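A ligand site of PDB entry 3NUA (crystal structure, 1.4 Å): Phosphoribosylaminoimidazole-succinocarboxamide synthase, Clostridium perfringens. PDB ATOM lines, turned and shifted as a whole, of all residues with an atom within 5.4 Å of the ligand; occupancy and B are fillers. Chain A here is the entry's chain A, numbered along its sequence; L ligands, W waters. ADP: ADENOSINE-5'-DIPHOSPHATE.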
ATOM      1  N   TYR A  12      15.979 -31.421 -24.183  1.00  0.00           N
ATOM      2  CA  TYR A  12      14.782 -30.728 -23.769  1.00  0.00           C
ATOM      3  C   TYR A  12      13.588 -31.198 -24.594  1.00  0.00           C
ATOM      4  O   TYR A  12      13.694 -31.309 -25.829  1.00  0.00           O
ATOM      5  CB  TYR A  12      14.986 -29.227 -24.007  1.00  0.00           C
ATOM      6  CG  TYR A  12      13.804 -28.334 -23.650  1.00  0.00           C
ATOM      7  CD1 TYR A  12      13.545 -27.994 -22.322  1.00  0.00           C
ATOM      8  CD2 TYR A  12      12.962 -27.838 -24.633  1.00  0.00           C
ATOM      9  CE1 TYR A  12      12.485 -27.181 -21.998  1.00  0.00           C
ATOM     10  CE2 TYR A  12      11.913 -27.008 -24.345  1.00  0.00           C
ATOM     11  CZ  TYR A  12      11.657 -26.690 -23.021  1.00  0.00           C
ATOM     12  OH  TYR A  12      10.626 -25.840 -22.698  1.00  0.00           O
ATOM     13  N   GLY A  14       9.964 -29.757 -25.464  1.00  0.00           N
ATOM     14  CA  GLY A  14       9.010 -28.653 -25.335  1.00  0.00           C
ATOM     15  C   GLY A  14       7.600 -29.076 -25.705  1.00  0.00           C
ATOM     16  O   GLY A  14       7.292 -30.275 -25.856  1.00  0.00           O
ATOM     17  N   LYS A  15       6.731 -28.083 -25.842  1.00  0.00           N
ATOM     18  CA  LYS A  15       5.340 -28.365 -26.170  1.00  0.00           C
ATOM     19  C   LYS A  15       5.182 -28.973 -27.552  1.00  0.00           C
ATOM     20  O   LYS A  15       4.240 -29.720 -27.769  1.00  0.00           O
ATOM     21  CB  LYS A  15       4.537 -27.073 -26.058  1.00  0.00           C
ATOM     22  CG  LYS A  15       4.491 -26.485 -24.629  1.00  0.00           C
ATOM     23  CD  LYS A  15       3.707 -25.134 -24.556  1.00  0.00           C
ATOM     24  CE  LYS A  15       4.294 -24.053 -25.454  1.00  0.00           C
ATOM     25  NZ  LYS A  15       5.660 -23.557 -25.063  1.00  0.00           N
ATOM     26  N   ALA A  16       6.064 -28.630 -28.485  1.00  0.00           N
ATOM     27  CA  ALA A  16       5.906 -29.041 -29.877  1.00  0.00           C
ATOM     28  C   ALA A  16       7.093 -29.776 -30.446  1.00  0.00           C
ATOM     29  O   ALA A  16       6.937 -30.560 -31.378  1.00  0.00           O
ATOM     30  CB  ALA A  16       5.594 -27.821 -30.733  1.00  0.00           C
ATOM     31  N   LYS A  17       8.304 -29.536 -29.911  1.00  0.00           N
ATOM     32  CA  LYS A  17       9.513 -30.152 -30.442  1.00  0.00           C
ATOM     33  C   LYS A  17      10.371 -30.723 -29.332  1.00  0.00           C
ATOM     34  O   LYS A  17      10.269 -30.295 -28.180  1.00  0.00           O
ATOM     35  CB  LYS A  17      10.339 -29.119 -31.223  1.00  0.00           C
ATOM     36  CG  LYS A  17       9.573 -28.557 -32.421  1.00  0.00           C
ATOM     37  CD  LYS A  17       9.060 -27.131 -32.161  1.00  0.00           C
ATOM     38  CE  LYS A  17      10.214 -26.093 -32.269  1.00  0.00           C
ATOM     39  NZ  LYS A  17       9.625 -24.816 -31.874  1.00  0.00           N
ATOM     40  N   LYS A  18      11.242 -31.668 -29.696  1.00  0.00           N
ATOM     41  CA  LYS A  18      12.332 -32.078 -28.813  1.00  0.00           C
ATOM     42  C   LYS A  18      13.639 -31.511 -29.383  1.00  0.00           C
ATOM     43  O   LYS A  18      13.804 -31.413 -30.616  1.00  0.00           O
ATOM     44  CB  LYS A  18      12.437 -33.610 -28.769  1.00  0.00           C
ATOM     45  CG  LYS A  18      11.239 -34.292 -28.119  1.00  0.00           C
ATOM     46  CD  LYS A  18      11.397 -35.822 -28.177  1.00  0.00           C
ATOM     47  CE  LYS A  18      10.318 -36.487 -27.376  1.00  0.00           C
ATOM     48  NZ  LYS A  18      10.421 -37.979 -27.563  1.00  0.00           N
ATOM     49  N   ILE A  19      14.542 -31.146 -28.485  1.00  0.00           N
ATOM     50  CA  ILE A  19      15.897 -30.729 -28.848  1.00  0.00           C
ATOM     51  C   ILE A  19      16.853 -31.833 -28.435  1.00  0.00           C
ATOM     52  O   ILE A  19      16.879 -32.181 -27.249  1.00  0.00           O
ATOM     53  CB  ILE A  19      16.295 -29.427 -28.153  1.00  0.00           C
ATOM     54  CG1 ILE A  19      15.296 -28.287 -28.442  1.00  0.00           C
ATOM     55  CG2 ILE A  19      17.733 -29.042 -28.506  1.00  0.00           C
ATOM     56  CD1 ILE A  19      15.250 -27.873 -29.936  1.00  0.00           C
ATOM     57  N   VAL A  28      22.540 -29.064 -32.618  1.00  0.00           N
ATOM     58  CA  VAL A  28      21.429 -29.837 -32.085  1.00  0.00           C
ATOM     59  C   VAL A  28      20.543 -30.344 -33.199  1.00  0.00           C
ATOM     60  O   VAL A  28      20.604 -29.843 -34.329  1.00  0.00           O
ATOM     61  CB  VAL A  28      20.550 -29.009 -31.093  1.00  0.00           C
ATOM     62  CG1 VAL A  28      21.347 -28.704 -29.826  1.00  0.00           C
ATOM     63  CG2 VAL A  28      19.983 -27.736 -31.764  1.00  0.00           C
ATOM     64  N   VAL A  30      16.556 -30.684 -34.024  1.00  0.00           N
ATOM     65  CA  VAL A  30      15.209 -30.256 -33.644  1.00  0.00           C
ATOM     66  C   VAL A  30      14.228 -31.239 -34.235  1.00  0.00           C
ATOM     67  O   VAL A  30      14.209 -31.424 -35.458  1.00  0.00           O
ATOM     68  CB  VAL A  30      14.880 -28.819 -34.142  1.00  0.00           C
ATOM     69  CG1 VAL A  30      13.502 -28.410 -33.627  1.00  0.00           C
ATOM     70  CG2 VAL A  30      15.963 -27.848 -33.665  1.00  0.00           C
ATOM     71  N   HIS A  73      19.998 -20.225 -37.328  1.00  0.00           N
ATOM     72  CA  HIS A  73      20.500 -21.492 -36.815  1.00  0.00           C
ATOM     73  C   HIS A  73      20.406 -22.658 -37.792  1.00  0.00           C
ATOM     74  O   HIS A  73      20.920 -23.749 -37.514  1.00  0.00           O
ATOM     75  CB  HIS A  73      19.820 -21.863 -35.496  1.00  0.00           C
ATOM     76  CG  HIS A  73      18.408 -22.363 -35.586  1.00  0.00           C
ATOM     77  ND1 HIS A  73      17.518 -22.171 -36.645  1.00  0.00           N
ATOM     78  CD2 HIS A  73      17.725 -23.035 -34.643  1.00  0.00           C
ATOM     79  CE1 HIS A  73      16.362 -22.754 -36.338  1.00  0.00           C
ATOM     80  NE2 HIS A  73      16.466 -23.276 -35.127  1.00  0.00           N
ATOM     81  N   CYS A  85      20.481 -28.028 -36.600  1.00  0.00           N
ATOM     82  CA  CYS A  85      20.652 -26.611 -36.335  1.00  0.00           C
ATOM     83  C   CYS A  85      21.856 -26.307 -35.472  1.00  0.00           C
ATOM     84  O   CYS A  85      22.289 -27.164 -34.709  1.00  0.00           O
ATOM     85  CB  CYS A  85      19.382 -26.065 -35.665  1.00  0.00           C
ATOM     86  SG  CYS A  85      17.899 -26.110 -36.669  1.00  0.00           S
ATOM     87  N   LYS A  86      22.388 -25.101 -35.584  1.00  0.00           N
ATOM     88  CA  LYS A  86      23.399 -24.657 -34.646  1.00  0.00           C
ATOM     89  C   LYS A  86      22.768 -24.582 -33.252  1.00  0.00           C
ATOM     90  O   LYS A  86      21.609 -24.122 -33.098  1.00  0.00           O
ATOM     91  CB  LYS A  86      23.896 -23.262 -35.049  1.00  0.00           C
ATOM     92  CG  LYS A  86      24.597 -23.302 -36.408  1.00  0.00           C
ATOM     93  CD  LYS A  86      24.920 -21.938 -36.949  1.00  0.00           C
ATOM     94  CE  LYS A  86      25.653 -22.088 -38.284  1.00  0.00           C
ATOM     95  NZ  LYS A  86      26.457 -20.912 -38.676  1.00  0.00           N
ATOM     96  N   LYS A  87      23.517 -24.996 -32.228  1.00  0.00           N
ATOM     97  CA  LYS A  87      23.051 -24.906 -30.857  1.00  0.00           C
ATOM     98  C   LYS A  87      23.243 -23.494 -30.365  1.00  0.00           C
ATOM     99  O   LYS A  87      24.370 -22.986 -30.372  1.00  0.00           O
ATOM    100  CB  LYS A  87      23.866 -25.866 -29.983  1.00  0.00           C
ATOM    101  CG  LYS A  87      23.358 -25.939 -28.545  1.00  0.00           C
ATOM    102  CD  LYS A  87      24.150 -26.904 -27.694  1.00  0.00           C
ATOM    103  CE  LYS A  87      23.527 -27.069 -26.336  1.00  0.00           C
ATOM    104  NZ  LYS A  87      24.403 -27.955 -25.504  1.00  0.00           N
ATOM    105  N   VAL A  88      22.156 -22.829 -30.024  1.00  0.00           N
ATOM    106  CA  VAL A  88      22.250 -21.440 -29.578  1.00  0.00           C
ATOM    107  C   VAL A  88      21.790 -21.291 -28.144  1.00  0.00           C
ATOM    108  O   VAL A  88      21.065 -22.136 -27.645  1.00  0.00           O
ATOM    109  CB  VAL A  88      21.450 -20.478 -30.499  1.00  0.00           C
ATOM    110  CG1 VAL A  88      21.830 -20.719 -31.964  1.00  0.00           C
ATOM    111  CG2 VAL A  88      19.942 -20.639 -30.273  1.00  0.00           C
ATOM    112  N   ILE A  90      19.258 -19.437 -26.287  1.00  0.00           N
ATOM    113  CA  ILE A  90      18.058 -18.686 -26.618  1.00  0.00           C
ATOM    114  C   ILE A  90      17.910 -17.458 -25.723  1.00  0.00           C
ATOM    115  O   ILE A  90      18.028 -17.534 -24.487  1.00  0.00           O
ATOM    116  CB  ILE A  90      16.805 -19.592 -26.522  1.00  0.00           C
ATOM    117  CG1 ILE A  90      16.868 -20.697 -27.604  1.00  0.00           C
ATOM    118  CG2 ILE A  90      15.504 -18.789 -26.653  1.00  0.00           C
ATOM    119  CD1 ILE A  90      16.536 -20.202 -29.016  1.00  0.00           C
ATOM    120  N   GLU A  94       9.884 -13.909 -26.682  1.00  0.00           N
ATOM    121  CA  GLU A  94       9.155 -14.170 -27.909  1.00  0.00           C
ATOM    122  C   GLU A  94       9.013 -12.824 -28.603  1.00  0.00           C
ATOM    123  O   GLU A  94       8.476 -11.900 -28.034  1.00  0.00           O
ATOM    124  CB  GLU A  94       7.755 -14.724 -27.605  1.00  0.00           C
ATOM    125  CG  GLU A  94       7.715 -15.843 -26.564  1.00  0.00           C
ATOM    126  CD  GLU A  94       8.210 -17.148 -27.085  1.00  0.00           C
ATOM    127  OE1 GLU A  94       7.532 -18.185 -26.915  1.00  0.00           O
ATOM    128  OE2 GLU A  94       9.304 -17.158 -27.655  1.00  0.00           O
ATOM    129  N   LYS A 127       9.620 -15.128 -22.264  1.00  0.00           N
ATOM    130  CA  LYS A 127       9.503 -16.577 -22.462  1.00  0.00           C
ATOM    131  C   LYS A 127       9.603 -17.286 -21.101  1.00  0.00           C
ATOM    132  O   LYS A 127      10.658 -17.705 -20.657  1.00  0.00           O
ATOM    133  CB  LYS A 127      10.538 -17.108 -23.446  1.00  0.00           C
ATOM    134  CG  LYS A 127      10.166 -18.525 -23.937  1.00  0.00           C
ATOM    135  CD  LYS A 127      11.058 -19.057 -25.065  1.00  0.00           C
ATOM    136  CE  LYS A 127      10.786 -20.535 -25.395  1.00  0.00           C
ATOM    137  NZ  LYS A 127       9.381 -20.718 -25.897  1.00  0.00           N
ATOM    138  N   ASP A 129       6.785 -19.854 -19.381  1.00  0.00           N
ATOM    139  CA  ASP A 129       5.443 -20.389 -19.481  1.00  0.00           C
ATOM    140  C   ASP A 129       4.712 -20.399 -18.118  1.00  0.00           C
ATOM    141  O   ASP A 129       3.481 -20.341 -18.073  1.00  0.00           O
ATOM    142  CB  ASP A 129       5.432 -21.783 -20.146  1.00  0.00           C
ATOM    143  CG  ASP A 129       5.817 -21.737 -21.652  1.00  0.00           C
ATOM    144  OD1 ASP A 129       6.002 -20.645 -22.228  1.00  0.00           O
ATOM    145  OD2 ASP A 129       5.941 -22.809 -22.282  1.00  0.00           O
ATOM    146  N   GLU A 183      12.041 -16.375 -32.382  1.00  0.00           N
ATOM    147  CA  GLU A 183      13.017 -16.391 -31.301  1.00  0.00           C
ATOM    148  C   GLU A 183      14.414 -16.311 -31.847  1.00  0.00           C
ATOM    149  O   GLU A 183      14.682 -16.743 -32.958  1.00  0.00           O
ATOM    150  CB  GLU A 183      12.899 -17.675 -30.468  1.00  0.00           C
ATOM    151  CG  GLU A 183      11.553 -17.846 -29.863  1.00  0.00           C
ATOM    152  CD  GLU A 183      11.412 -19.099 -29.065  1.00  0.00           C
ATOM    153  OE1 GLU A 183      12.355 -19.946 -29.026  1.00  0.00           O
ATOM    154  OE2 GLU A 183      10.298 -19.275 -28.494  1.00  0.00           O
ATOM    155  N   ALA A 194      16.450 -18.294 -34.576  1.00  0.00           N
ATOM    156  CA  ALA A 194      16.417 -19.715 -34.201  1.00  0.00           C
ATOM    157  C   ALA A 194      14.994 -20.198 -34.162  1.00  0.00           C
ATOM    158  O   ALA A 194      14.108 -19.636 -34.799  1.00  0.00           O
ATOM    159  CB  ALA A 194      17.139 -19.920 -32.882  1.00  0.00           C
ATOM    160  N   ASP A 195      14.762 -21.312 -33.471  1.00  0.00           N
ATOM    161  CA  ASP A 195      13.408 -21.867 -33.340  1.00  0.00           C
ATOM    162  C   ASP A 195      12.736 -22.165 -34.701  1.00  0.00           C
ATOM    163  O   ASP A 195      13.334 -22.832 -35.544  1.00  0.00           O
ATOM    164  CB  ASP A 195      12.538 -21.042 -32.375  1.00  0.00           C
ATOM    165  CG  ASP A 195      11.343 -21.801 -31.879  1.00  0.00           C
ATOM    166  OD1 ASP A 195      11.557 -22.906 -31.325  1.00  0.00           O
ATOM    167  OD2 ASP A 195      10.225 -21.339 -32.042  1.00  0.00           O
ATOM    168  N   GLU A 196      11.487 -21.751 -34.871  1.00  0.00           N
ATOM    169  CA  GLU A 196      10.571 -22.241 -35.900  1.00  0.00           C
ATOM    170  C   GLU A 196       9.833 -21.087 -36.568  1.00  0.00           C
ATOM    171  O   GLU A 196       9.579 -20.072 -35.915  1.00  0.00           O
ATOM    172  CB  GLU A 196       9.588 -23.146 -35.150  1.00  0.00           C
ATOM    173  CG  GLU A 196       8.336 -23.537 -35.846  1.00  0.00           C
ATOM    174  CD  GLU A 196       7.410 -24.352 -34.967  1.00  0.00           C
ATOM    175  OE1 GLU A 196       7.547 -24.422 -33.696  1.00  0.00           O
ATOM    176  OE2 GLU A 196       6.494 -24.919 -35.558  1.00  0.00           O
HETATM  177  PB  ADP L   1       8.780 -24.540 -25.748  1.00  0.00           P
HETATM  178  O1B ADP L   1       9.872 -24.302 -24.719  1.00  0.00           O
HETATM  179  O2B ADP L   1       8.339 -23.270 -26.414  1.00  0.00           O
HETATM  180  O3B ADP L   1       7.613 -25.407 -25.215  1.00  0.00           O
HETATM  181  PA  ADP L   1       9.271 -25.967 -28.321  1.00  0.00           P
HETATM  182  O1A ADP L   1       8.352 -27.143 -28.289  1.00  0.00           O
HETATM  183  O2A ADP L   1       9.011 -24.791 -29.199  1.00  0.00           O
HETATM  184  O3A ADP L   1       9.560 -25.485 -26.796  1.00  0.00           O
HETATM  185  O5' ADP L   1      10.718 -26.539 -28.688  1.00  0.00           O
HETATM  186  C5' ADP L   1      11.872 -25.810 -29.021  1.00  0.00           C
HETATM  187  C4' ADP L   1      12.625 -25.346 -27.781  1.00  0.00           C
HETATM  188  O4' ADP L   1      13.979 -25.258 -28.200  1.00  0.00           O
HETATM  189  C3' ADP L   1      12.218 -23.955 -27.323  1.00  0.00           C
HETATM  190  O3' ADP L   1      12.440 -23.797 -25.908  1.00  0.00           O
HETATM  191  C2' ADP L   1      13.224 -23.085 -28.069  1.00  0.00           C
HETATM  192  O2' ADP L   1      13.478 -21.801 -27.481  1.00  0.00           O
HETATM  193  C1' ADP L   1      14.478 -23.929 -28.076  1.00  0.00           C
HETATM  194  N9  ADP L   1      15.310 -23.724 -29.279  1.00  0.00           N
HETATM  195  C8  ADP L   1      14.903 -23.386 -30.524  1.00  0.00           C
HETATM  196  N7  ADP L   1      15.948 -23.367 -31.399  1.00  0.00           N
HETATM  197  C5  ADP L   1      17.038 -23.724 -30.658  1.00  0.00           C
HETATM  198  C6  ADP L   1      18.459 -23.900 -30.932  1.00  0.00           C
HETATM  199  N6  ADP L   1      18.966 -23.739 -32.194  1.00  0.00           N
HETATM  200  N1  ADP L   1      19.267 -24.242 -29.912  1.00  0.00           N
HETATM  201  C2  ADP L   1      18.796 -24.438 -28.657  1.00  0.00           C
HETATM  202  N3  ADP L   1      17.494 -24.314 -28.314  1.00  0.00           N
HETATM  203  C4  ADP L   1      16.612 -23.931 -29.281  1.00  0.00           C
HETATM  204  O   HOH W   1       5.968 -24.718 -29.037  1.00  0.00           O
HETATM  205  O   HOH W   2       7.831 -26.428 -22.732  1.00  0.00           O
HETATM  206  O   HOH W   3       7.756 -22.133 -31.061  1.00  0.00           O
HETATM  207  O   HOH W   4      14.170 -21.547 -24.688  1.00  0.00           O
HETATM  208  O   HOH W   5       9.158 -22.361 -22.960  1.00  0.00           O
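Merely in contact with the ligand: Gly 14 (3.3 Å), Ile 19 (3.3 Å), His 73 (2.8 Å), Lys 87 (3.96 Å), Ile 90 (3.6 Å) and Ala 194 (3.9 Å). Of the 22 residues printed, 15 come within 4 Å of the ligand. The nearest printed residue that does not touch the ligand is Val 28 (4.02 Å).
The backbone NH of Lys 15 sits at hydrogen-bond distance from an oxygen (O3B) of the ligand (2.9 Å). NZ of Lys 17 lies within salt-bridge range of O2A of the ligand, at 2.7 Å. The backbone NH (N) of Asp 195 lies within hydrogen-bond range of a nitrogen (N7) of the ligand (3.2 Å). A nitrogen (N6) of the ligand lies within hydrogen-bond range of the backbone carbonyl oxygen of Lys 86. An oxygen (O1B) of the ligand lies within hydrogen-bond range of the side-chain hydroxyl of Tyr 12, at 2.6 Å. The backbone NH of Ala 16 lies within hydrogen-bond range of an oxygen (O1A) of the ligand (2.7 Å). OE1 of Glu 183 sits at hydrogen-bond distance from O2' of the ligand (2.7 Å). NZ of Lys 15 lies within salt-bridge range of O3B of the ligand (2.7 Å). The backbone NH (N) of Val 88 lies within hydrogen-bond range of a nitrogen (N1) of the ligand, 3.2 Å away. An oxygen (O2B) of the ligand is in salt-bridge range of the side-chain amino group (NZ) of Lys 127 (2.8 Å). N of Lys 17 sits at hydrogen-bond distance from O1A of the ligand (2.9 Å).
The backbone carbonyl oxygen (O) of Glu 183 sits at hydrogen-bond distance from the backbone NH (N) of Ala 194 (2.9 Å). The side-chain carboxylate (OE1) of Glu 196 lies within salt-bridge range of the side-chain amino group (NZ) of Lys 17. OE1 of Glu 94 lies within salt-bridge range of NZ of Lys 127, 3.3 Å away. The side-chain amino group (NZ) of Lys 17 is in salt-bridge range of the side-chain carboxylate (OD1) of Asp 195 (2.8 Å). N of Ile 19 sits at hydrogen-bond distance from O of Tyr 12, 2.8 Å away. The side-chain carboxylate of Glu 183 is in salt-bridge range of the side-chain amino group of Lys 127 (3.1 Å). NE2 of His 73 sits at hydrogen-bond distance from N of Asp 195, 3.1 Å away. A ring nitrogen (NE2) of His 73 is in hydrogen-bond range of the side-chain sulfur (SG) of Cys 85, at 3.5 Å.
Water W2 bridges O3B of the ligand (2.7 Å) and OH of Tyr 12 (2.9 Å). Water W5 lies within hydrogen-bond range of O1B of the ligand (2.7 Å), OD2 of Asp 129 (3.3 Å) and NZ of Lys 127 (3.4 Å). Water W3 lies within hydrogen-bond range of the side-chain carboxylate (OD2) of Asp 195, the side-chain amino group (NZ) of Lys 17, an oxygen (O2A) of the ligand and the side-chain carboxylate (OE1) of Glu 196.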
